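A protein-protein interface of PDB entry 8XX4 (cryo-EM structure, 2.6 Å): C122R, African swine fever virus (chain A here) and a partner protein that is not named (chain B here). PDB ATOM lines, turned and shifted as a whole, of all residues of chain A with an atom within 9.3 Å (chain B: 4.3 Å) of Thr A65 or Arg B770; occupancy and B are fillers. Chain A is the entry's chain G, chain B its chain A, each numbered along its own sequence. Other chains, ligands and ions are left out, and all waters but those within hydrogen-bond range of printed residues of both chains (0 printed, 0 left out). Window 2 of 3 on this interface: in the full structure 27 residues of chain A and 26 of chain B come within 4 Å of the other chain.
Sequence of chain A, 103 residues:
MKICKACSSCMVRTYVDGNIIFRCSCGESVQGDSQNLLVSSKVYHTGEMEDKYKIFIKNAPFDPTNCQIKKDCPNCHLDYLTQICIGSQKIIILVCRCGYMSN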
ATOM      1  N   PHE A  56      20.652 -28.580 -39.937  1.00  0.00           N
ATOM      2  CA  PHE A  56      21.197 -27.949 -38.742  1.00  0.00           C
ATOM      3  C   PHE A  56      21.937 -26.664 -39.077  1.00  0.00           C
ATOM      4  O   PHE A  56      21.838 -25.679 -38.345  1.00  0.00           O
ATOM      5  CB  PHE A  56      22.123 -28.912 -38.009  1.00  0.00           C
ATOM      6  CG  PHE A  56      22.882 -28.273 -36.892  1.00  0.00           C
ATOM      7  CD1 PHE A  56      22.235 -27.888 -35.735  1.00  0.00           C
ATOM      8  CD2 PHE A  56      24.238 -28.038 -37.002  1.00  0.00           C
ATOM      9  CE1 PHE A  56      22.925 -27.293 -34.708  1.00  0.00           C
ATOM     10  CE2 PHE A  56      24.930 -27.441 -35.978  1.00  0.00           C
ATOM     11  CZ  PHE A  56      24.273 -27.068 -34.832  1.00  0.00           C
ATOM     12  N   ASN A  59      19.431 -23.992 -39.703  1.00  0.00           N
ATOM     13  CA  ASN A  59      18.748 -23.559 -38.491  1.00  0.00           C
ATOM     14  C   ASN A  59      19.675 -22.918 -37.466  1.00  0.00           C
ATOM     15  O   ASN A  59      19.181 -22.305 -36.518  1.00  0.00           O
ATOM     16  CB  ASN A  59      18.033 -24.744 -37.840  1.00  0.00           C
ATOM     17  CG  ASN A  59      16.855 -25.227 -38.646  1.00  0.00           C
ATOM     18  OD1 ASN A  59      16.182 -24.446 -39.312  1.00  0.00           O
ATOM     19  ND2 ASN A  59      16.593 -26.523 -38.585  1.00  0.00           N
ATOM     20  N   ALA A  60      20.990 -23.047 -37.633  1.00  0.00           N
ATOM     21  CA  ALA A  60      21.930 -22.606 -36.604  1.00  0.00           C
ATOM     22  C   ALA A  60      21.761 -21.153 -36.176  1.00  0.00           C
ATOM     23  O   ALA A  60      21.797 -20.890 -34.963  1.00  0.00           O
ATOM     24  CB  ALA A  60      23.361 -22.874 -37.076  1.00  0.00           C
ATOM     25  N   PRO A  61      21.603 -20.175 -37.072  1.00  0.00           N
ATOM     26  CA  PRO A  61      21.480 -18.787 -36.600  1.00  0.00           C
ATOM     27  C   PRO A  61      20.262 -18.543 -35.734  1.00  0.00           C
ATOM     28  O   PRO A  61      20.243 -17.563 -34.982  1.00  0.00           O
ATOM     29  CB  PRO A  61      21.410 -17.977 -37.897  1.00  0.00           C
ATOM     30  CG  PRO A  61      21.968 -18.853 -38.925  1.00  0.00           C
ATOM     31  CD  PRO A  61      21.610 -20.233 -38.542  1.00  0.00           C
ATOM     32  N   PHE A  62      19.245 -19.395 -35.814  1.00  0.00           N
ATOM     33  CA  PHE A  62      18.025 -19.219 -35.043  1.00  0.00           C
ATOM     34  C   PHE A  62      17.999 -20.041 -33.764  1.00  0.00           C
ATOM     35  O   PHE A  62      17.170 -19.773 -32.893  1.00  0.00           O
ATOM     36  CB  PHE A  62      16.813 -19.560 -35.913  1.00  0.00           C
ATOM     37  CG  PHE A  62      16.821 -18.859 -37.236  1.00  0.00           C
ATOM     38  CD1 PHE A  62      16.336 -17.570 -37.350  1.00  0.00           C
ATOM     39  CD2 PHE A  62      17.343 -19.473 -38.357  1.00  0.00           C
ATOM     40  CE1 PHE A  62      16.356 -16.918 -38.559  1.00  0.00           C
ATOM     41  CE2 PHE A  62      17.365 -18.823 -39.566  1.00  0.00           C
ATOM     42  CZ  PHE A  62      16.870 -17.546 -39.667  1.00  0.00           C
ATOM     43  N   ASP A  63      18.879 -21.014 -33.628  1.00  0.00           N
ATOM     44  CA  ASP A  63      19.003 -21.737 -32.374  1.00  0.00           C
ATOM     45  C   ASP A  63      19.686 -20.835 -31.358  1.00  0.00           C
ATOM     46  O   ASP A  63      20.833 -20.426 -31.581  1.00  0.00           O
ATOM     47  CB  ASP A  63      19.805 -23.015 -32.589  1.00  0.00           C
ATOM     48  CG  ASP A  63      19.639 -24.010 -31.465  1.00  0.00           C
ATOM     49  OD1 ASP A  63      18.766 -23.805 -30.600  1.00  0.00           O
ATOM     50  OD2 ASP A  63      20.382 -25.011 -31.449  1.00  0.00           O
ATOM     51  N   PRO A  64      19.034 -20.488 -30.245  1.00  0.00           N
ATOM     52  CA  PRO A  64      19.676 -19.597 -29.268  1.00  0.00           C
ATOM     53  C   PRO A  64      20.812 -20.248 -28.507  1.00  0.00           C
ATOM     54  O   PRO A  64      21.604 -19.531 -27.883  1.00  0.00           O
ATOM     55  CB  PRO A  64      18.530 -19.208 -28.324  1.00  0.00           C
ATOM     56  CG  PRO A  64      17.300 -19.859 -28.850  1.00  0.00           C
ATOM     57  CD  PRO A  64      17.691 -20.907 -29.824  1.00  0.00           C
ATOM     58  N   THR A  65      20.924 -21.571 -28.541  1.00  0.00           N
ATOM     59  CA  THR A  65      21.959 -22.285 -27.815  1.00  0.00           C
ATOM     60  C   THR A  65      23.258 -22.416 -28.594  1.00  0.00           C
ATOM     61  O   THR A  65      24.222 -22.975 -28.066  1.00  0.00           O
ATOM     62  CB  THR A  65      21.459 -23.675 -27.433  1.00  0.00           C
ATOM     63  OG1 THR A  65      21.730 -24.586 -28.502  1.00  0.00           O
ATOM     64  CG2 THR A  65      19.979 -23.637 -27.192  1.00  0.00           C
ATOM     65  N   ASN A  66      23.308 -21.926 -29.827  1.00  0.00           N
ATOM     66  CA  ASN A  66      24.530 -21.968 -30.609  1.00  0.00           C
ATOM     67  C   ASN A  66      25.461 -20.830 -30.218  1.00  0.00           C
ATOM     68  O   ASN A  66      25.024 -19.734 -29.857  1.00  0.00           O
ATOM     69  CB  ASN A  66      24.215 -21.887 -32.100  1.00  0.00           C
ATOM     70  CG  ASN A  66      23.936 -23.238 -32.708  1.00  0.00           C
ATOM     71  OD1 ASN A  66      22.873 -23.467 -33.274  1.00  0.00           O
ATOM     72  ND2 ASN A  66      24.893 -24.142 -32.594  1.00  0.00           N
ATOM     73  N   CYS A  67      26.759 -21.100 -30.300  1.00  0.00           N
ATOM     74  CA  CYS A  67      27.760 -20.097 -29.971  1.00  0.00           C
ATOM     75  C   CYS A  67      27.765 -18.974 -31.002  1.00  0.00           C
ATOM     76  O   CYS A  67      27.463 -19.176 -32.179  1.00  0.00           O
ATOM     77  CB  CYS A  67      29.144 -20.739 -29.893  1.00  0.00           C
ATOM     78  SG  CYS A  67      30.299 -19.896 -28.801  1.00  0.00           S
ATOM     79  N   GLN A  68      28.110 -17.775 -30.543  1.00  0.00           N
ATOM     80  CA  GLN A  68      28.261 -16.616 -31.409  1.00  0.00           C
ATOM     81  C   GLN A  68      29.624 -15.985 -31.171  1.00  0.00           C
ATOM     82  O   GLN A  68      30.191 -16.088 -30.081  1.00  0.00           O
ATOM     83  CB  GLN A  68      27.167 -15.578 -31.167  1.00  0.00           C
ATOM     84  CG  GLN A  68      25.835 -16.164 -30.776  1.00  0.00           C
ATOM     85  CD  GLN A  68      24.862 -16.193 -31.924  1.00  0.00           C
ATOM     86  OE1 GLN A  68      24.840 -15.289 -32.752  1.00  0.00           O
ATOM     87  NE2 GLN A  68      24.046 -17.234 -31.982  1.00  0.00           N
ATOM     88  N   THR A  82      26.952 -16.753 -36.035  1.00  0.00           N
ATOM     89  CA  THR A  82      26.803 -18.037 -35.368  1.00  0.00           C
ATOM     90  C   THR A  82      27.951 -18.953 -35.759  1.00  0.00           C
ATOM     91  O   THR A  82      28.267 -19.097 -36.941  1.00  0.00           O
ATOM     92  CB  THR A  82      25.465 -18.673 -35.730  1.00  0.00           C
ATOM     93  OG1 THR A  82      24.403 -17.797 -35.342  1.00  0.00           O
ATOM     94  CG2 THR A  82      25.300 -20.001 -35.020  1.00  0.00           C
ATOM     95  N   GLN A  83      28.573 -19.577 -34.766  1.00  0.00           N
ATOM     96  CA  GLN A  83      29.741 -20.415 -34.976  1.00  0.00           C
ATOM     97  C   GLN A  83      29.363 -21.880 -34.819  1.00  0.00           C
ATOM     98  O   GLN A  83      28.743 -22.263 -33.823  1.00  0.00           O
ATOM     99  CB  GLN A  83      30.849 -20.049 -33.993  1.00  0.00           C
ATOM    100  CG  GLN A  83      32.235 -20.326 -34.505  1.00  0.00           C
ATOM    101  CD  GLN A  83      33.262 -20.271 -33.408  1.00  0.00           C
ATOM    102  OE1 GLN A  83      34.233 -19.523 -33.490  1.00  0.00           O
ATOM    103  NE2 GLN A  83      33.055 -21.063 -32.364  1.00  0.00           N
ATOM    104  N   CYS A  85      30.966 -25.913 -35.119  1.00  0.00           N
ATOM    105  CA  CYS A  85      32.174 -26.735 -35.137  1.00  0.00           C
ATOM    106  C   CYS A  85      31.725 -28.187 -35.271  1.00  0.00           C
ATOM    107  O   CYS A  85      31.561 -28.893 -34.274  1.00  0.00           O
ATOM    108  CB  CYS A  85      33.010 -26.507 -33.887  1.00  0.00           C
ATOM    109  SG  CYS A  85      34.732 -26.988 -34.054  1.00  0.00           S
ATOM    110  N   PRO B 764      30.721 -33.629 -24.531  1.00  0.00           N
ATOM    111  CA  PRO B 764      29.418 -32.968 -24.746  1.00  0.00           C
ATOM    112  C   PRO B 764      28.242 -33.943 -24.715  1.00  0.00           C
ATOM    113  O   PRO B 764      27.715 -34.392 -25.728  1.00  0.00           O
ATOM    114  CB  PRO B 764      29.595 -32.322 -26.121  1.00  0.00           C
ATOM    115  CG  PRO B 764      30.607 -33.154 -26.800  1.00  0.00           C
ATOM    116  CD  PRO B 764      31.557 -33.606 -25.740  1.00  0.00           C
ATOM    117  N   GLN B 765      27.814 -34.274 -23.497  1.00  0.00           N
ATOM    118  CA  GLN B 765      26.757 -35.251 -23.275  1.00  0.00           C
ATOM    119  C   GLN B 765      25.369 -34.638 -23.165  1.00  0.00           C
ATOM    120  O   GLN B 765      24.380 -35.361 -23.317  1.00  0.00           O
ATOM    121  CB  GLN B 765      27.041 -36.048 -21.998  1.00  0.00           C
ATOM    122  CG  GLN B 765      26.928 -37.547 -22.159  1.00  0.00           C
ATOM    123  CD  GLN B 765      27.887 -38.090 -23.188  1.00  0.00           C
ATOM    124  OE1 GLN B 765      29.103 -37.967 -23.044  1.00  0.00           O
ATOM    125  NE2 GLN B 765      27.347 -38.689 -24.241  1.00  0.00           N
ATOM    126  N   PHE B 766      25.269 -33.336 -22.894  1.00  0.00           N
ATOM    127  CA  PHE B 766      23.962 -32.724 -22.673  1.00  0.00           C
ATOM    128  C   PHE B 766      23.126 -32.737 -23.943  1.00  0.00           C
ATOM    129  O   PHE B 766      21.967 -33.164 -23.937  1.00  0.00           O
ATOM    130  CB  PHE B 766      24.138 -31.296 -22.162  1.00  0.00           C
ATOM    131  CG  PHE B 766      22.852 -30.553 -21.999  1.00  0.00           C
ATOM    132  CD1 PHE B 766      21.989 -30.860 -20.970  1.00  0.00           C
ATOM    133  CD2 PHE B 766      22.506 -29.548 -22.873  1.00  0.00           C
ATOM    134  CE1 PHE B 766      20.809 -30.179 -20.819  1.00  0.00           C
ATOM    135  CE2 PHE B 766      21.326 -28.867 -22.724  1.00  0.00           C
ATOM    136  CZ  PHE B 766      20.478 -29.182 -21.694  1.00  0.00           C
ATOM    137  N   SER B 767      23.701 -32.271 -25.041  1.00  0.00           N
ATOM    138  CA  SER B 767      23.028 -32.230 -26.324  1.00  0.00           C
ATOM    139  C   SER B 767      24.102 -32.367 -27.393  1.00  0.00           C
ATOM    140  O   SER B 767      25.251 -32.704 -27.096  1.00  0.00           O
ATOM    141  CB  SER B 767      22.202 -30.943 -26.452  1.00  0.00           C
ATOM    142  OG  SER B 767      21.654 -30.806 -27.748  1.00  0.00           O
ATOM    143  N   PHE B 768      23.735 -32.113 -28.642  1.00  0.00           N
ATOM    144  CA  PHE B 768      24.708 -32.180 -29.725  1.00  0.00           C
ATOM    145  C   PHE B 768      25.677 -31.014 -29.594  1.00  0.00           C
ATOM    146  O   PHE B 768      25.325 -29.873 -29.895  1.00  0.00           O
ATOM    147  CB  PHE B 768      24.004 -32.159 -31.075  1.00  0.00           C
ATOM    148  CG  PHE B 768      24.936 -32.005 -32.238  1.00  0.00           C
ATOM    149  CD1 PHE B 768      26.013 -32.855 -32.396  1.00  0.00           C
ATOM    150  CD2 PHE B 768      24.737 -31.006 -33.173  1.00  0.00           C
ATOM    151  CE1 PHE B 768      26.873 -32.713 -33.461  1.00  0.00           C
ATOM    152  CE2 PHE B 768      25.592 -30.862 -34.242  1.00  0.00           C
ATOM    153  CZ  PHE B 768      26.662 -31.715 -34.384  1.00  0.00           C
ATOM    154  N   GLY B 769      26.894 -31.293 -29.140  1.00  0.00           N
ATOM    155  CA  GLY B 769      27.901 -30.263 -28.997  1.00  0.00           C
ATOM    156  C   GLY B 769      27.832 -29.455 -27.724  1.00  0.00           C
ATOM    157  O   GLY B 769      28.570 -28.472 -27.596  1.00  0.00           O
ATOM    158  N   ARG B 770      26.977 -29.836 -26.777  1.00  0.00           N
ATOM    159  CA  ARG B 770      26.791 -29.108 -25.530  1.00  0.00           C
ATOM    160  C   ARG B 770      27.213 -29.982 -24.360  1.00  0.00           C
ATOM    161  O   ARG B 770      26.851 -31.159 -24.303  1.00  0.00           O
ATOM    162  CB  ARG B 770      25.334 -28.689 -25.349  1.00  0.00           C
ATOM    163  CG  ARG B 770      24.848 -27.665 -26.334  1.00  0.00           C
ATOM    164  CD  ARG B 770      23.487 -27.154 -25.932  1.00  0.00           C
ATOM    165  NE  ARG B 770      23.588 -26.128 -24.906  1.00  0.00           N
ATOM    166  CZ  ARG B 770      22.550 -25.575 -24.301  1.00  0.00           C
ATOM    167  NH1 ARG B 770      21.314 -25.946 -24.575  1.00  0.00           N
ATOM    168  NH2 ARG B 770      22.757 -24.625 -23.398  1.00  0.00           N
ATOM    169  N   THR B 771      27.961 -29.401 -23.426  1.00  0.00           N
ATOM    170  CA  THR B 771      28.340 -30.108 -22.210  1.00  0.00           C
ATOM    171  C   THR B 771      27.322 -29.917 -21.094  1.00  0.00           C
ATOM    172  O   THR B 771      27.049 -30.853 -20.339  1.00  0.00           O
ATOM    173  CB  THR B 771      29.714 -29.639 -21.733  1.00  0.00           C
ATOM    174  OG1 THR B 771      29.801 -28.216 -21.862  1.00  0.00           O
ATOM    175  CG2 THR B 771      30.804 -30.268 -22.562  1.00  0.00           C
ATOM    176  N   LEU B 772      26.758 -28.719 -20.980  1.00  0.00           N
ATOM    177  CA  LEU B 772      25.785 -28.403 -19.947  1.00  0.00           C
ATOM    178  C   LEU B 772      24.803 -27.396 -20.517  1.00  0.00           C
ATOM    179  O   LEU B 772      25.059 -26.769 -21.546  1.00  0.00           O
ATOM    180  CB  LEU B 772      26.453 -27.839 -18.687  1.00  0.00           C
ATOM    181  CG  LEU B 772      26.996 -28.807 -17.636  1.00  0.00           C
ATOM    182  CD1 LEU B 772      27.561 -28.036 -16.472  1.00  0.00           C
ATOM    183  CD2 LEU B 772      25.914 -29.748 -17.166  1.00  0.00           C
ATOM    184  N   VAL B 773      23.667 -27.246 -19.835  1.00  0.00           N
ATOM    185  CA  VAL B 773      22.678 -26.263 -20.254  1.00  0.00           C
ATOM    186  C   VAL B 773      23.204 -24.843 -20.093  1.00  0.00           C
ATOM    187  O   VAL B 773      22.648 -23.908 -20.676  1.00  0.00           O
ATOM    188  CB  VAL B 773      21.365 -26.477 -19.473  1.00  0.00           C
ATOM    189  CG1 VAL B 773      21.518 -26.042 -18.032  1.00  0.00           C
ATOM    190  CG2 VAL B 773      20.210 -25.755 -20.141  1.00  0.00           C
ATOM    191  N   TYR B 775      26.238 -23.799 -21.055  1.00  0.00           N
ATOM    192  CA  TYR B 775      27.207 -23.420 -22.056  1.00  0.00           C
ATOM    193  C   TYR B 775      26.625 -23.594 -23.448  1.00  0.00           C
ATOM    194  O   TYR B 775      25.862 -24.533 -23.687  1.00  0.00           O
ATOM    195  CB  TYR B 775      28.480 -24.257 -21.919  1.00  0.00           C
ATOM    196  CG  TYR B 775      29.161 -24.056 -20.593  1.00  0.00           C
ATOM    197  CD1 TYR B 775      29.804 -22.864 -20.303  1.00  0.00           C
ATOM    198  CD2 TYR B 775      29.143 -25.044 -19.626  1.00  0.00           C
ATOM    199  CE1 TYR B 775      30.418 -22.669 -19.096  1.00  0.00           C
ATOM    200  CE2 TYR B 775      29.758 -24.857 -18.415  1.00  0.00           C
ATOM    201  CZ  TYR B 775      30.394 -23.668 -18.156  1.00  0.00           C
ATOM    202  OH  TYR B 775      31.010 -23.474 -16.946  1.00  0.00           O
ATOM    203  N   PRO B 776      26.957 -22.708 -24.380  1.00  0.00           N
ATOM    204  CA  PRO B 776      26.345 -22.773 -25.705  1.00  0.00           C
ATOM    205  C   PRO B 776      26.852 -23.972 -26.484  1.00  0.00           C
ATOM    206  O   PRO B 776      27.815 -24.642 -26.115  1.00  0.00           O
ATOM    207  CB  PRO B 776      26.769 -21.455 -26.351  1.00  0.00           C
ATOM    208  CG  PRO B 776      28.026 -21.112 -25.683  1.00  0.00           C
ATOM    209  CD  PRO B 776      27.905 -21.590 -24.271  1.00  0.00           C
ATOM    210  N   ARG B 777      26.157 -24.250 -27.578  1.00  0.00           N
ATOM    211  CA  ARG B 777      26.560 -25.331 -28.459  1.00  0.00           C
ATOM    212  C   ARG B 777      27.887 -25.002 -29.125  1.00  0.00           C
ATOM    213  O   ARG B 777      28.098 -23.884 -29.599  1.00  0.00           O
ATOM    214  CB  ARG B 777      25.483 -25.572 -29.507  1.00  0.00           C
ATOM    215  CG  ARG B 777      25.664 -26.829 -30.292  1.00  0.00           C
ATOM    216  CD  ARG B 777      24.450 -27.102 -31.136  1.00  0.00           C
ATOM    217  NE  ARG B 777      23.550 -28.036 -30.476  1.00  0.00           N
ATOM    218  CZ  ARG B 777      22.263 -27.808 -30.274  1.00  0.00           C
ATOM    219  NH1 ARG B 777      21.688 -26.691 -30.684  1.00  0.00           N
ATOM    220  NH2 ARG B 777      21.534 -28.724 -29.646  1.00  0.00           N
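Of the 13 printed residues of chain B, 4 touch a printed residue of chain A.
Printed residues of chain B that touch a printed residue of chain A: Phe B768, Arg B770, Pro B776 and Arg B777.
Of the 14 printed residues of chain A, 5 touch a printed residue of chain B.
Hydrophobic or aromatic side chains of chain A within 4 Å of the printed part of chain B: Phe A56.
Along chain A the printed residues that touch a printed residue of chain B span positions 56 to 67.
Among the printed residues, Asp or Glu carboxylates within 4 Å of a Lys or Arg side-chain nitrogen of the other chain: Asp A63 with Arg B777 (2.3 Å).
OG1 of Thr A65 is in hydrogen-bond range of NH1 of Arg B777, 3.0 Å away.
NH1 of Arg B777 lies close to OD2 of Asp A63 (2.3 Å).
The backbone NH (N) of Cys A67 lies within hydrogen-bond range of the backbone carbonyl oxygen (O) of Arg B777.
Asn A59 touches none of the printed residues of chain B.
Thr A65 touches just these residues of chain B: Arg B770 (3.7 Å), Pro B776 (3.2 Å) and Arg B777 (2.4 Å).
Of the printed residues of chain B, Asn A66 touches Arg B777 (3.3 Å).
No residue of chain A comes within 4 Å of Ser B767.
Of the printed residues of chain A, Phe B768 touches Phe A56 (3.9 Å).
No residue of chain A comes within 4 Å of Gly B769.
Arg B770 touches one residue of chain A.
No residue of chain A comes within 4 Å of Thr B771.
Arg B777 touches just these residues of chain A: Phe A56, Asp A63, Thr A65, Asn A66 and Cys A67.
The nearest residue of chain A that does not touch Arg B770 is Asn A66 (6.5 Å).
O of Val B773 is in hydrogen-bond range of NH2 of Arg B770 (2.8 Å).
The side-chain amide oxygen (OD1) of Asn A66 lies close to the backbone carbonyl oxygen (O) of Ala A60 (3.3 Å).
The backbone carbonyl oxygen (O) of Arg B770 is in hydrogen-bond range of the backbone NH (N) of Gln B765, 3.4 Å away.
The backbone carbonyl oxygen (O) of Asn A66 lies within hydrogen-bond range of the side-chain amide nitrogen (NE2) of Gln A68 (3.4 Å).
OD2 of Asp A63 is in hydrogen-bond range of OG1 of Thr A65.
O of Cys A67 lies within hydrogen-bond range of N of Gln A83, 2.8 Å away.
Phe A56 touches Phe B768.
CZ of Phe A56 touches CD of Arg B777, 3.7 Å away.
CB of Thr A65 touches NH1 of Arg B770, at 3.7 Å.
Thr A65 touches Pro B776 (O to CA, 3.2 Å).
Asn A66 touches Arg B777 (ND2 to CD, 3.3 Å).
N of Cys A67 touches CB of Pro B776, at 3.96 Å.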
